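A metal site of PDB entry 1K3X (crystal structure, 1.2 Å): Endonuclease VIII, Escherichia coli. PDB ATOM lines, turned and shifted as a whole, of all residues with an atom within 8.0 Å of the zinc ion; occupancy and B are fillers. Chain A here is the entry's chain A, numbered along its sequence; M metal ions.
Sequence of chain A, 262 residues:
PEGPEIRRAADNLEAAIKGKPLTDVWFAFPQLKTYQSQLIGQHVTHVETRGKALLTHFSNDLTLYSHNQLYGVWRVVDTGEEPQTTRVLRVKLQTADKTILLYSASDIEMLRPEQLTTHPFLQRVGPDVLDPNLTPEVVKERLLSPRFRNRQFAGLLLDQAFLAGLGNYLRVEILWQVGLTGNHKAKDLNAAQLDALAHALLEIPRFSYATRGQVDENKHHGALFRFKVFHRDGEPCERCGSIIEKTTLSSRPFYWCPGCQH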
ATOM      1  N   TRP A 176     -19.654  -8.788  18.451  1.00  0.00           N
ATOM      2  CA  TRP A 176     -20.670  -9.792  18.105  1.00  0.00           C
ATOM      3  C   TRP A 176     -21.025 -10.605  19.324  1.00  0.00           C
ATOM      4  O   TRP A 176     -22.213 -10.895  19.568  1.00  0.00           O
ATOM      5  CB  TRP A 176     -20.129 -10.713  16.998  1.00  0.00           C
ATOM      6  CG  TRP A 176     -21.131 -11.791  16.609  1.00  0.00           C
ATOM      7  CD1 TRP A 176     -22.094 -11.713  15.644  1.00  0.00           C
ATOM      8  CD2 TRP A 176     -21.232 -13.096  17.186  1.00  0.00           C
ATOM      9  NE1 TRP A 176     -22.793 -12.910  15.570  1.00  0.00           N
ATOM     10  CE2 TRP A 176     -22.292 -13.765  16.509  1.00  0.00           C
ATOM     11  CE3 TRP A 176     -20.563 -13.763  18.201  1.00  0.00           C
ATOM     12  CZ2 TRP A 176     -22.664 -15.061  16.839  1.00  0.00           C
ATOM     13  CZ3 TRP A 176     -20.935 -15.072  18.523  1.00  0.00           C
ATOM     14  CH2 TRP A 176     -21.987 -15.704  17.828  1.00  0.00           C
ATOM     15  N   VAL A 229     -17.562 -14.052  13.229  1.00  0.00           N
ATOM     16  CA  VAL A 229     -17.991 -13.166  12.130  1.00  0.00           C
ATOM     17  C   VAL A 229     -16.788 -12.655  11.349  1.00  0.00           C
ATOM     18  O   VAL A 229     -16.967 -12.327  10.150  1.00  0.00           O
ATOM     19  CB  VAL A 229     -18.866 -11.960  12.541  1.00  0.00           C
ATOM     20  CG1 VAL A 229     -20.250 -12.470  13.026  1.00  0.00           C
ATOM     21  CG2 VAL A 229     -18.229 -11.073  13.574  1.00  0.00           C
ATOM     22  N   PRO A 236     -24.034 -17.546   6.936  1.00  0.00           N
ATOM     23  CA  PRO A 236     -25.029 -17.371   7.955  1.00  0.00           C
ATOM     24  C   PRO A 236     -24.378 -17.301   9.329  1.00  0.00           C
ATOM     25  O   PRO A 236     -23.489 -18.060   9.720  1.00  0.00           O
ATOM     26  CB  PRO A 236     -25.934 -18.626   7.894  1.00  0.00           C
ATOM     27  CG  PRO A 236     -25.316 -19.484   6.881  1.00  0.00           C
ATOM     28  CD  PRO A 236     -24.072 -18.885   6.316  1.00  0.00           C
ATOM     29  N   CYS A 237     -24.890 -16.330  10.090  1.00  0.00           N
ATOM     30  CA  CYS A 237     -24.537 -16.226  11.509  1.00  0.00           C
ATOM     31  C   CYS A 237     -24.870 -17.499  12.261  1.00  0.00           C
ATOM     32  O   CYS A 237     -25.977 -17.995  12.163  1.00  0.00           O
ATOM     33  CB  CYS A 237     -25.331 -15.055  12.076  1.00  0.00           C
ATOM     34  SG  CYS A 237     -25.173 -14.798  13.874  1.00  0.00           S
ATOM     35  N   GLU A 238     -23.928 -17.972  13.084  1.00  0.00           N
ATOM     36  CA  GLU A 238     -24.253 -19.202  13.796  1.00  0.00           C
ATOM     37  C   GLU A 238     -25.268 -19.000  14.920  1.00  0.00           C
ATOM     38  O   GLU A 238     -25.824 -20.003  15.405  1.00  0.00           O
ATOM     39  CB  GLU A 238     -22.981 -19.829  14.313  1.00  0.00           C
ATOM     40  CG  GLU A 238     -22.318 -19.077  15.425  1.00  0.00           C
ATOM     41  CD  GLU A 238     -21.036 -19.851  15.789  1.00  0.00           C
ATOM     42  OE1 GLU A 238     -20.972 -20.362  16.914  1.00  0.00           O
ATOM     43  OE2 GLU A 238     -20.129 -19.965  14.957  1.00  0.00           O
ATOM     44  N   ARG A 239     -25.560 -17.753  15.309  1.00  0.00           N
ATOM     45  CA  ARG A 239     -26.530 -17.485  16.364  1.00  0.00           C
ATOM     46  C   ARG A 239     -27.952 -17.306  15.826  1.00  0.00           C
ATOM     47  O   ARG A 239     -28.870 -17.928  16.366  1.00  0.00           O
ATOM     48  CB  ARG A 239     -26.115 -16.226  17.167  1.00  0.00           C
ATOM     49  CG  ARG A 239     -27.081 -15.873  18.274  1.00  0.00           C
ATOM     50  CD  ARG A 239     -26.358 -15.150  19.389  1.00  0.00           C
ATOM     51  NE  ARG A 239     -25.770 -13.976  18.936  1.00  0.00           N
ATOM     52  CZ  ARG A 239     -24.778 -13.211  19.358  1.00  0.00           C
ATOM     53  NH1 ARG A 239     -24.030 -13.479  20.426  1.00  0.00           N
ATOM     54  NH2 ARG A 239     -24.540 -12.122  18.664  1.00  0.00           N
ATOM     55  N   CYS A 240     -28.090 -16.491  14.767  1.00  0.00           N
ATOM     56  CA  CYS A 240     -29.474 -16.204  14.346  1.00  0.00           C
ATOM     57  C   CYS A 240     -29.690 -16.563  12.873  1.00  0.00           C
ATOM     58  O   CYS A 240     -30.820 -16.419  12.398  1.00  0.00           O
ATOM     59  CB  CYS A 240     -29.803 -14.713  14.562  1.00  0.00           C
ATOM     60  SG  CYS A 240     -28.937 -13.626  13.393  1.00  0.00           S
ATOM     61  N   GLY A 241     -28.664 -16.941  12.134  1.00  0.00           N
ATOM     62  CA  GLY A 241     -28.853 -17.300  10.752  1.00  0.00           C
ATOM     63  C   GLY A 241     -28.888 -16.205   9.746  1.00  0.00           C
ATOM     64  O   GLY A 241     -28.876 -16.463   8.523  1.00  0.00           O
ATOM     65  N   SER A 242     -28.900 -14.931  10.140  1.00  0.00           N
ATOM     66  CA  SER A 242     -28.819 -13.853   9.168  1.00  0.00           C
ATOM     67  C   SER A 242     -27.454 -13.879   8.473  1.00  0.00           C
ATOM     68  O   SER A 242     -26.476 -14.423   9.049  1.00  0.00           O
ATOM     69  CB  SER A 242     -29.058 -12.463   9.792  1.00  0.00           C
ATOM     70  OG  SER A 242     -30.416 -12.297  10.211  1.00  0.00           O
ATOM     71  N   ILE A 243     -27.370 -13.274   7.282  1.00  0.00           N
ATOM     72  CA  ILE A 243     -26.111 -13.292   6.555  1.00  0.00           C
ATOM     73  C   ILE A 243     -25.194 -12.165   7.031  1.00  0.00           C
ATOM     74  O   ILE A 243     -25.525 -10.989   7.096  1.00  0.00           O
ATOM     75  CB  ILE A 243     -26.391 -13.188   5.054  1.00  0.00           C
ATOM     76  CG1 ILE A 243     -27.319 -14.294   4.519  1.00  0.00           C
ATOM     77  CG2 ILE A 243     -25.042 -13.206   4.321  1.00  0.00           C
ATOM     78  CD1 ILE A 243     -26.824 -15.712   4.720  1.00  0.00           C
ATOM     79  N   ILE A 244     -23.988 -12.613   7.426  1.00  0.00           N
ATOM     80  CA  ILE A 244     -22.993 -11.711   7.989  1.00  0.00           C
ATOM     81  C   ILE A 244     -22.582 -10.726   6.905  1.00  0.00           C
ATOM     82  O   ILE A 244     -22.435 -11.133   5.737  1.00  0.00           O
ATOM     83  CB  ILE A 244     -21.794 -12.530   8.495  1.00  0.00           C
ATOM     84  CG1 ILE A 244     -22.214 -13.391   9.702  1.00  0.00           C
ATOM     85  CG2 ILE A 244     -20.612 -11.686   8.873  1.00  0.00           C
ATOM     86  CD1 ILE A 244     -21.318 -14.592   9.919  1.00  0.00           C
ATOM     87  N   TRP A 256     -20.158  -7.957  10.810  1.00  0.00           N
ATOM     88  CA  TRP A 256     -21.181  -7.952  11.849  1.00  0.00           C
ATOM     89  C   TRP A 256     -22.409  -8.654  11.302  1.00  0.00           C
ATOM     90  O   TRP A 256     -22.557  -8.850  10.096  1.00  0.00           O
ATOM     91  CB  TRP A 256     -21.506  -6.500  12.259  1.00  0.00           C
ATOM     92  CG  TRP A 256     -22.127  -5.748  11.131  1.00  0.00           C
ATOM     93  CD1 TRP A 256     -21.606  -5.390   9.908  1.00  0.00           C
ATOM     94  CD2 TRP A 256     -23.470  -5.265  11.166  1.00  0.00           C
ATOM     95  NE1 TRP A 256     -22.523  -4.694   9.167  1.00  0.00           N
ATOM     96  CE2 TRP A 256     -23.710  -4.596   9.922  1.00  0.00           C
ATOM     97  CE3 TRP A 256     -24.488  -5.319  12.126  1.00  0.00           C
ATOM     98  CZ2 TRP A 256     -24.937  -4.010   9.628  1.00  0.00           C
ATOM     99  CZ3 TRP A 256     -25.709  -4.720  11.812  1.00  0.00           C
ATOM    100  CH2 TRP A 256     -25.935  -4.084  10.590  1.00  0.00           C
ATOM    101  N   CYS A 257     -23.300  -9.024  12.211  1.00  0.00           N
ATOM    102  CA  CYS A 257     -24.566  -9.649  11.889  1.00  0.00           C
ATOM    103  C   CYS A 257     -25.755  -8.720  12.097  1.00  0.00           C
ATOM    104  O   CYS A 257     -25.979  -8.276  13.224  1.00  0.00           O
ATOM    105  CB  CYS A 257     -24.757 -10.927  12.709  1.00  0.00           C
ATOM    106  SG  CYS A 257     -26.356 -11.650  12.205  1.00  0.00           S
ATOM    107  N   PRO A 258     -26.510  -8.431  11.021  1.00  0.00           N
ATOM    108  CA  PRO A 258     -27.670  -7.532  11.169  1.00  0.00           C
ATOM    109  C   PRO A 258     -28.823  -8.128  11.935  1.00  0.00           C
ATOM    110  O   PRO A 258     -29.740  -7.385  12.300  1.00  0.00           O
ATOM    111  CB  PRO A 258     -28.025  -7.225   9.696  1.00  0.00           C
ATOM    112  CG  PRO A 258     -27.678  -8.523   8.999  1.00  0.00           C
ATOM    113  CD  PRO A 258     -26.330  -8.892   9.606  1.00  0.00           C
ATOM    114  N   GLY A 259     -28.802  -9.441  12.159  1.00  0.00           N
ATOM    115  CA  GLY A 259     -29.946 -10.035  12.869  1.00  0.00           C
ATOM    116  C   GLY A 259     -29.759 -10.029  14.386  1.00  0.00           C
ATOM    117  O   GLY A 259     -30.771 -10.126  15.095  1.00  0.00           O
ATOM    118  N   CYS A 260     -28.523  -9.927  14.863  1.00  0.00           N
ATOM    119  CA  CYS A 260     -28.349 -10.077  16.324  1.00  0.00           C
ATOM    120  C   CYS A 260     -27.367  -9.060  16.916  1.00  0.00           C
ATOM    121  O   CYS A 260     -27.075  -9.159  18.104  1.00  0.00           O
ATOM    122  CB  CYS A 260     -27.965 -11.515  16.671  1.00  0.00           C
ATOM    123  SG  CYS A 260     -26.364 -12.030  16.019  1.00  0.00           S
ATOM    124  N   GLN A 261     -26.872  -8.120  16.111  1.00  0.00           N
ATOM    125  CA  GLN A 261     -26.093  -7.003  16.664  1.00  0.00           C
ATOM    126  C   GLN A 261     -26.905  -5.725  16.506  1.00  0.00           C
ATOM    127  O   GLN A 261     -27.379  -5.414  15.393  1.00  0.00           O
ATOM    128  CB  GLN A 261     -24.711  -6.872  15.997  1.00  0.00           C
ATOM    129  CG  GLN A 261     -23.789  -8.012  16.435  1.00  0.00           C
ATOM    130  CD  GLN A 261     -22.451  -7.891  15.746  1.00  0.00           C
ATOM    131  OE1 GLN A 261     -22.233  -8.646  14.768  1.00  0.00           O
ATOM    132  NE2 GLN A 261     -21.548  -7.009  16.200  1.00  0.00           N
ATOM    133  N   HIS A 262     -27.056  -4.984  17.596  1.00  0.00           N
ATOM    134  CA  HIS A 262     -27.895  -3.810  17.618  1.00  0.00           C
ATOM    135  C   HIS A 262     -27.180  -2.634  18.255  1.00  0.00           C
ATOM    136  O   HIS A 262     -27.688  -1.538  17.994  1.00  0.00           O
ATOM    137  CB  HIS A 262     -29.170  -4.041  18.437  1.00  0.00           C
ATOM    138  CG  HIS A 262     -29.856  -5.252  17.919  1.00  0.00           C
ATOM    139  ND1 HIS A 262     -30.553  -5.328  16.745  1.00  0.00           N
ATOM    140  CD2 HIS A 262     -29.843  -6.493  18.401  1.00  0.00           C
ATOM    141  CE1 HIS A 262     -31.014  -6.566  16.522  1.00  0.00           C
ATOM    142  NE2 HIS A 262     -30.571  -7.261  17.557  1.00  0.00           N
ATOM    143  OXT HIS A 262     -26.215  -2.838  18.994  1.00  0.00           O
HETATM  144 ZN    ZN M   1     -26.782 -13.066  14.001  1.00  0.00          ZN
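Four residues have an atom within 4 Å of the zinc ion: Cys 237, Cys 240, Cys 257 and Cys 260.
The zinc ion is bound by the side-chain sulfur (SG) of Cys 260 (2.3 Å), the side-chain sulfur (SG) of Cys 240 (2.3 Å), the side-chain sulfur (SG) of Cys 257 (2.3 Å) and the side-chain sulfur (SG) of Cys 237 (2.4 Å). The zinc ion has four donor atoms within binding distance.
The indole nitrogen (NE1) of Trp 176 sits close to the side-chain sulfur (SG) of Cys 237 (3.5 Å). The side-chain sulfur (SG) of Cys 240 sits close to the backbone NH (N) of Ser 242 (3.5 Å). The side-chain sulfur of Cys 260 sits close to the indole nitrogen of Trp 176 (3.7 Å). SG of Cys 257 lies close to N of Gly 259 (3.3 Å). SG of Cys 260 sits close to NH2 of Arg 239. N of Arg 239 lies close to SG of Cys 237 (3.3 Å). The side-chain amide oxygen of Gln 261 sits at hydrogen-bond distance from the backbone NH of Cys 257 (2.8 Å). N of Cys 237 lies within hydrogen-bond range of O of Ser 242 (2.7 Å).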
